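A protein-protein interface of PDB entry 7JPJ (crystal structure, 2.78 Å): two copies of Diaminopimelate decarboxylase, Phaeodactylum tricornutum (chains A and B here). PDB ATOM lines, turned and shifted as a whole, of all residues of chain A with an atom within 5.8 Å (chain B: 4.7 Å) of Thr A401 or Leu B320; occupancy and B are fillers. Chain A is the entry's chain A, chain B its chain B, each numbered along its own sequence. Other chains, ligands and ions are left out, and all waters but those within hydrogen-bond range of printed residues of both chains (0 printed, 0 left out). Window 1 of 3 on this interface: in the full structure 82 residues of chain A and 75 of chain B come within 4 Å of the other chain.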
ATOM      1  N   MET A 316       7.723 -10.926  -7.165  1.00  0.00           N
ATOM      2  CA  MET A 316       7.267 -12.304  -7.325  1.00  0.00           C
ATOM      3  C   MET A 316       8.413 -13.309  -7.241  1.00  0.00           C
ATOM      4  O   MET A 316       8.165 -14.493  -6.987  1.00  0.00           O
ATOM      5  CB  MET A 316       6.529 -12.454  -8.654  1.00  0.00           C
ATOM      6  CG  MET A 316       7.213 -11.740  -9.802  1.00  0.00           C
ATOM      7  SD  MET A 316       6.548 -12.205 -11.405  1.00  0.00           S
ATOM      8  CE  MET A 316       4.800 -11.904 -11.143  1.00  0.00           C
ATOM      9  N   THR A 317       9.655 -12.863  -7.456  1.00  0.00           N
ATOM     10  CA  THR A 317      10.823 -13.694  -7.187  1.00  0.00           C
ATOM     11  C   THR A 317      10.904 -14.120  -5.726  1.00  0.00           C
ATOM     12  O   THR A 317      11.568 -15.114  -5.415  1.00  0.00           O
ATOM     13  CB  THR A 317      12.100 -12.940  -7.559  1.00  0.00           C
ATOM     14  OG1 THR A 317      12.004 -11.589  -7.086  1.00  0.00           O
ATOM     15  CG2 THR A 317      12.304 -12.930  -9.062  1.00  0.00           C
ATOM     16  N   ASP A 318      10.254 -13.392  -4.829  1.00  0.00           N
ATOM     17  CA  ASP A 318      10.342 -13.656  -3.399  1.00  0.00           C
ATOM     18  C   ASP A 318       8.997 -13.929  -2.748  1.00  0.00           C
ATOM     19  O   ASP A 318       8.913 -14.774  -1.853  1.00  0.00           O
ATOM     20  CB  ASP A 318      11.025 -12.476  -2.702  1.00  0.00           C
ATOM     21  CG  ASP A 318      12.212 -11.959  -3.486  1.00  0.00           C
ATOM     22  OD1 ASP A 318      13.270 -12.627  -3.480  1.00  0.00           O
ATOM     23  OD2 ASP A 318      12.078 -10.900  -4.133  1.00  0.00           O
ATOM     24  N   LEU A 320       5.200 -14.742  -4.231  1.00  0.00           N
ATOM     25  CA  LEU A 320       4.373 -14.957  -5.409  1.00  0.00           C
ATOM     26  C   LEU A 320       2.880 -14.946  -5.109  1.00  0.00           C
ATOM     27  O   LEU A 320       2.081 -14.745  -6.031  1.00  0.00           O
ATOM     28  CB  LEU A 320       4.750 -16.290  -6.071  1.00  0.00           C
ATOM     29  CG  LEU A 320       3.950 -16.760  -7.288  1.00  0.00           C
ATOM     30  CD1 LEU A 320       4.241 -15.895  -8.505  1.00  0.00           C
ATOM     31  CD2 LEU A 320       4.223 -18.226  -7.573  1.00  0.00           C
ATOM     32  N   LEU A 324      -0.230 -14.870  -7.673  1.00  0.00           N
ATOM     33  CA  LEU A 324      -0.818 -16.171  -7.971  1.00  0.00           C
ATOM     34  C   LEU A 324      -2.274 -16.260  -7.530  1.00  0.00           C
ATOM     35  O   LEU A 324      -3.091 -16.889  -8.211  1.00  0.00           O
ATOM     36  CB  LEU A 324       0.006 -17.279  -7.315  1.00  0.00           C
ATOM     37  CG  LEU A 324      -0.355 -18.711  -7.709  1.00  0.00           C
ATOM     38  CD1 LEU A 324      -0.390 -18.863  -9.224  1.00  0.00           C
ATOM     39  CD2 LEU A 324       0.633 -19.686  -7.094  1.00  0.00           C
ATOM     40  N   MET A 399       8.008 -21.355  -2.227  1.00  0.00           N
ATOM     41  CA  MET A 399       7.236 -21.405  -3.462  1.00  0.00           C
ATOM     42  C   MET A 399       7.180 -20.028  -4.112  1.00  0.00           C
ATOM     43  O   MET A 399       6.226 -19.269  -3.914  1.00  0.00           O
ATOM     44  CB  MET A 399       5.825 -21.939  -3.196  1.00  0.00           C
ATOM     45  CG  MET A 399       4.883 -21.870  -4.392  1.00  0.00           C
ATOM     46  SD  MET A 399       3.146 -21.856  -3.914  1.00  0.00           S
ATOM     47  CE  MET A 399       2.762 -20.123  -4.151  1.00  0.00           C
ATOM     48  N   SER A 400       8.210 -19.693  -4.880  1.00  0.00           N
ATOM     49  CA  SER A 400       8.275 -18.423  -5.580  1.00  0.00           C
ATOM     50  C   SER A 400       8.996 -18.640  -6.901  1.00  0.00           C
ATOM     51  O   SER A 400       9.531 -19.718  -7.171  1.00  0.00           O
ATOM     52  CB  SER A 400       8.989 -17.351  -4.745  1.00  0.00           C
ATOM     53  OG  SER A 400      10.336 -17.715  -4.487  1.00  0.00           O
ATOM     54  N   THR A 401       9.011 -17.602  -7.725  1.00  0.00           N
ATOM     55  CA  THR A 401       9.724 -17.651  -9.001  1.00  0.00           C
ATOM     56  C   THR A 401      11.123 -17.057  -8.847  1.00  0.00           C
ATOM     57  O   THR A 401      11.469 -16.032  -9.433  1.00  0.00           O
ATOM     58  CB  THR A 401       8.925 -16.933 -10.085  1.00  0.00           C
ATOM     59  OG1 THR A 401       8.634 -15.596  -9.664  1.00  0.00           O
ATOM     60  CG2 THR A 401       7.624 -17.665 -10.349  1.00  0.00           C
ATOM     61  N   LYS A 402      11.926 -17.730  -8.026  1.00  0.00           N
ATOM     62  CA  LYS A 402      13.312 -17.331  -7.837  1.00  0.00           C
ATOM     63  C   LYS A 402      14.063 -17.382  -9.163  1.00  0.00           C
ATOM     64  O   LYS A 402      13.762 -18.193 -10.044  1.00  0.00           O
ATOM     65  CB  LYS A 402      13.991 -18.240  -6.811  1.00  0.00           C
ATOM     66  CG  LYS A 402      14.175 -19.674  -7.282  1.00  0.00           C
ATOM     67  CD  LYS A 402      14.826 -20.544  -6.221  1.00  0.00           C
ATOM     68  CE  LYS A 402      13.790 -21.110  -5.270  1.00  0.00           C
ATOM     69  NZ  LYS A 402      14.377 -22.116  -4.341  1.00  0.00           N
ATOM     70  N   ASN A 403      15.035 -16.482  -9.305  1.00  0.00           N
ATOM     71  CA  ASN A 403      15.941 -16.366 -10.443  1.00  0.00           C
ATOM     72  C   ASN A 403      15.253 -15.872 -11.713  1.00  0.00           C
ATOM     73  O   ASN A 403      15.915 -15.760 -12.752  1.00  0.00           O
ATOM     74  CB  ASN A 403      16.675 -17.684 -10.733  1.00  0.00           C
ATOM     75  CG  ASN A 403      17.390 -18.229  -9.508  1.00  0.00           C
ATOM     76  OD1 ASN A 403      17.394 -19.435  -9.259  1.00  0.00           O
ATOM     77  ND2 ASN A 403      17.992 -17.338  -8.732  1.00  0.00           N
ATOM     78  N   TYR A 404      13.956 -15.574 -11.670  1.00  0.00           N
ATOM     79  CA  TYR A 404      13.331 -14.819 -12.748  1.00  0.00           C
ATOM     80  C   TYR A 404      13.978 -13.444 -12.841  1.00  0.00           C
ATOM     81  O   TYR A 404      14.241 -12.798 -11.821  1.00  0.00           O
ATOM     82  CB  TYR A 404      11.829 -14.688 -12.496  1.00  0.00           C
ATOM     83  CG  TYR A 404      11.070 -13.967 -13.586  1.00  0.00           C
ATOM     84  CD1 TYR A 404      11.371 -14.175 -14.925  1.00  0.00           C
ATOM     85  CD2 TYR A 404      10.045 -13.081 -13.275  1.00  0.00           C
ATOM     86  CE1 TYR A 404      10.678 -13.522 -15.925  1.00  0.00           C
ATOM     87  CE2 TYR A 404       9.343 -12.423 -14.269  1.00  0.00           C
ATOM     88  CZ  TYR A 404       9.667 -12.647 -15.593  1.00  0.00           C
ATOM     89  OH  TYR A 404       8.975 -11.995 -16.589  1.00  0.00           O
ATOM     90  N   MET B 316       3.744 -27.162 -11.685  1.00  0.00           N
ATOM     91  CA  MET B 316       4.000 -25.727 -11.616  1.00  0.00           C
ATOM     92  C   MET B 316       5.461 -25.426 -11.315  1.00  0.00           C
ATOM     93  O   MET B 316       5.913 -24.301 -11.558  1.00  0.00           O
ATOM     94  CB  MET B 316       3.112 -25.075 -10.556  1.00  0.00           C
ATOM     95  CG  MET B 316       3.161 -25.770  -9.211  1.00  0.00           C
ATOM     96  SD  MET B 316       1.971 -25.112  -8.025  1.00  0.00           S
ATOM     97  CE  MET B 316       2.017 -23.362  -8.414  1.00  0.00           C
ATOM     98  N   ASP B 318       7.739 -26.496 -13.028  1.00  0.00           N
ATOM     99  CA  ASP B 318       8.367 -26.496 -14.340  1.00  0.00           C
ATOM    100  C   ASP B 318       7.647 -25.619 -15.350  1.00  0.00           C
ATOM    101  O   ASP B 318       8.303 -24.925 -16.132  1.00  0.00           O
ATOM    102  CB  ASP B 318       8.449 -27.937 -14.856  1.00  0.00           C
ATOM    103  CG  ASP B 318       8.965 -28.896 -13.798  1.00  0.00           C
ATOM    104  OD1 ASP B 318      10.199 -28.972 -13.608  1.00  0.00           O
ATOM    105  OD2 ASP B 318       8.133 -29.557 -13.134  1.00  0.00           O
ATOM    106  N   VAL B 319       6.315 -25.626 -15.360  1.00  0.00           N
ATOM    107  CA  VAL B 319       5.517 -24.763 -16.225  1.00  0.00           C
ATOM    108  C   VAL B 319       4.444 -24.110 -15.361  1.00  0.00           C
ATOM    109  O   VAL B 319       3.511 -24.784 -14.906  1.00  0.00           O
ATOM    110  CB  VAL B 319       4.887 -25.529 -17.398  1.00  0.00           C
ATOM    111  CG1 VAL B 319       4.194 -24.564 -18.348  1.00  0.00           C
ATOM    112  CG2 VAL B 319       5.945 -26.324 -18.144  1.00  0.00           C
ATOM    113  N   LEU B 320       4.574 -22.800 -15.137  1.00  0.00           N
ATOM    114  CA  LEU B 320       3.691 -22.064 -14.243  1.00  0.00           C
ATOM    115  C   LEU B 320       2.556 -21.347 -14.963  1.00  0.00           C
ATOM    116  O   LEU B 320       1.527 -21.075 -14.337  1.00  0.00           O
ATOM    117  CB  LEU B 320       4.499 -21.038 -13.435  1.00  0.00           C
ATOM    118  CG  LEU B 320       3.771 -20.151 -12.422  1.00  0.00           C
ATOM    119  CD1 LEU B 320       3.195 -20.980 -11.278  1.00  0.00           C
ATOM    120  CD2 LEU B 320       4.695 -19.066 -11.895  1.00  0.00           C
ATOM    121  N   ARG B 321       2.713 -21.053 -16.252  1.00  0.00           N
ATOM    122  CA  ARG B 321       1.707 -20.285 -16.984  1.00  0.00           C
ATOM    123  C   ARG B 321       0.284 -20.823 -16.857  1.00  0.00           C
ATOM    124  O   ARG B 321      -0.647 -20.001 -16.801  1.00  0.00           O
ATOM    125  CB  ARG B 321       2.115 -20.184 -18.463  1.00  0.00           C
ATOM    126  CG  ARG B 321       3.410 -19.423 -18.689  1.00  0.00           C
ATOM    127  CD  ARG B 321       3.678 -19.175 -20.168  1.00  0.00           C
ATOM    128  NE  ARG B 321       2.920 -18.041 -20.696  1.00  0.00           N
ATOM    129  CZ  ARG B 321       1.963 -18.140 -21.614  1.00  0.00           C
ATOM    130  NH1 ARG B 321       1.638 -19.325 -22.115  1.00  0.00           N
ATOM    131  NH2 ARG B 321       1.328 -17.053 -22.033  1.00  0.00           N
ATOM    132  N   PRO B 322       0.031 -22.139 -16.818  1.00  0.00           N
ATOM    133  CA  PRO B 322      -1.352 -22.584 -16.564  1.00  0.00           C
ATOM    134  C   PRO B 322      -1.913 -22.089 -15.239  1.00  0.00           C
ATOM    135  O   PRO B 322      -3.038 -21.579 -15.202  1.00  0.00           O
ATOM    136  CB  PRO B 322      -1.236 -24.113 -16.618  1.00  0.00           C
ATOM    137  CG  PRO B 322      -0.100 -24.360 -17.535  1.00  0.00           C
ATOM    138  CD  PRO B 322       0.884 -23.259 -17.261  1.00  0.00           C
ATOM    139  N   SER B 323      -1.158 -22.212 -14.144  1.00  0.00           N
ATOM    140  CA  SER B 323      -1.662 -21.745 -12.855  1.00  0.00           C
ATOM    141  C   SER B 323      -1.654 -20.224 -12.757  1.00  0.00           C
ATOM    142  O   SER B 323      -2.536 -19.634 -12.123  1.00  0.00           O
ATOM    143  CB  SER B 323      -0.842 -22.349 -11.713  1.00  0.00           C
ATOM    144  OG  SER B 323      -0.451 -23.678 -12.008  1.00  0.00           O
ATOM    145  N   LEU B 324      -0.670 -19.569 -13.374  1.00  0.00           N
ATOM    146  CA  LEU B 324      -0.513 -18.131 -13.193  1.00  0.00           C
ATOM    147  C   LEU B 324      -1.515 -17.335 -14.023  1.00  0.00           C
ATOM    148  O   LEU B 324      -2.030 -16.312 -13.559  1.00  0.00           O
ATOM    149  CB  LEU B 324       0.920 -17.718 -13.536  1.00  0.00           C
ATOM    150  CG  LEU B 324       1.364 -16.292 -13.201  1.00  0.00           C
ATOM    151  CD1 LEU B 324       1.162 -15.982 -11.725  1.00  0.00           C
ATOM    152  CD2 LEU B 324       2.819 -16.090 -13.592  1.00  0.00           C
ATOM    153  N   MET B 399      10.955 -18.904 -15.544  1.00  0.00           N
ATOM    154  CA  MET B 399       9.928 -18.334 -14.667  1.00  0.00           C
ATOM    155  C   MET B 399       9.046 -19.490 -14.185  1.00  0.00           C
ATOM    156  O   MET B 399       8.035 -19.810 -14.812  1.00  0.00           O
ATOM    157  CB  MET B 399       9.117 -17.274 -15.383  1.00  0.00           C
ATOM    158  CG  MET B 399       8.422 -16.284 -14.462  1.00  0.00           C
ATOM    159  SD  MET B 399       6.752 -15.882 -15.013  1.00  0.00           S
ATOM    160  CE  MET B 399       7.077 -14.805 -16.403  1.00  0.00           C
ATOM    161  N   SER B 400       9.443 -20.101 -13.068  1.00  0.00           N
ATOM    162  CA  SER B 400       8.715 -21.224 -12.499  1.00  0.00           C
ATOM    163  C   SER B 400       8.938 -21.243 -10.994  1.00  0.00           C
ATOM    164  O   SER B 400       9.828 -20.570 -10.468  1.00  0.00           O
ATOM    165  CB  SER B 400       9.158 -22.557 -13.112  1.00  0.00           C
ATOM    166  OG  SER B 400      10.558 -22.736 -12.973  1.00  0.00           O
ATOM    167  N   THR B 401       8.120 -22.032 -10.306  1.00  0.00           N
ATOM    168  CA  THR B 401       8.255 -22.228  -8.864  1.00  0.00           C
ATOM    169  C   THR B 401       9.134 -23.434  -8.562  1.00  0.00           C
ATOM    170  O   THR B 401       8.749 -24.329  -7.812  1.00  0.00           O
ATOM    171  CB  THR B 401       6.882 -22.392  -8.224  1.00  0.00           C
ATOM    172  OG1 THR B 401       6.196 -23.488  -8.841  1.00  0.00           O
ATOM    173  CG2 THR B 401       6.060 -21.137  -8.409  1.00  0.00           C
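Thr A401 touches just these residues of chain B: Leu B320 and Ser B400. Of chain A, only Thr A401 (3.6 Å) comes within 4 Å of Leu B320. Printed residues of chain A within 4 Å of Ser B323: Leu A324. Printed residues of chain B within 4 Å of Leu A324: Ser B323 (3.7 Å). Of the printed residues of chain A, Met B399 touches Tyr A404. Printed residues of chain B within 4 Å of Ser A400: Ser B400 and Thr B401. Of the printed residues of chain A, Ser B400 touches Ser A400 (3.4 Å) and Thr A401 (3.3 Å). The nearest residue of chain B that does not touch Thr A401 is Thr B401 (4.3 Å). The nearest printed residue of chain A that does not touch Thr B401 is Met A399 (4.2 Å).
Printed residues of chain A that touch a printed residue of chain B: Leu A320, Leu A324, Ser A400, Thr A401 and Tyr A404. Hydrophobic or aromatic side chains of chain A within 4 Å of the printed part of chain B: Leu A320, Leu A324 and Tyr A404. Among the printed residues, 7 pairs touch across the chains.
O of Ser A400 lies close to O of Ser B400 (3.4 Å).
Leu A320 touches Thr B401, and with the chains exchanged Thr A401 touches Leu B320. Ser B400 touches its own counterpart, Ser A400. Ser A400 touches Thr B401, and with the chains exchanged Thr A401 touches Ser B400. Positions printed for both chains: 316, 318, 320, 324, 399, 400 and 401. Of the 7 pairs that touch across the chains among the printed residues, 5 have their exchanged pair printed and touching as well.
The backbone carbonyl oxygen (O) of Met A316 sits at hydrogen-bond distance from the side-chain hydroxyl (OG1) of Thr A401 (2.9 Å). The side-chain hydroxyl of Ser A400 lies within hydrogen-bond range of the backbone carbonyl oxygen of Thr A317, at 3.0 Å. OG1 of Thr B401 is in hydrogen-bond range of O of Met B316, at 2.9 Å.
Among the printed residues, merely in contact across the chains: Thr A401 with Ser B400 (3.3 Å), Ser A400 with Thr B401 (3.3 Å), Tyr A404 with Met B399 (3.4 Å), Leu A320 with Thr B401 (3.5 Å), Thr A401 with Leu B320 (3.6 Å) and Leu A324 with Ser B323 (3.7 Å).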
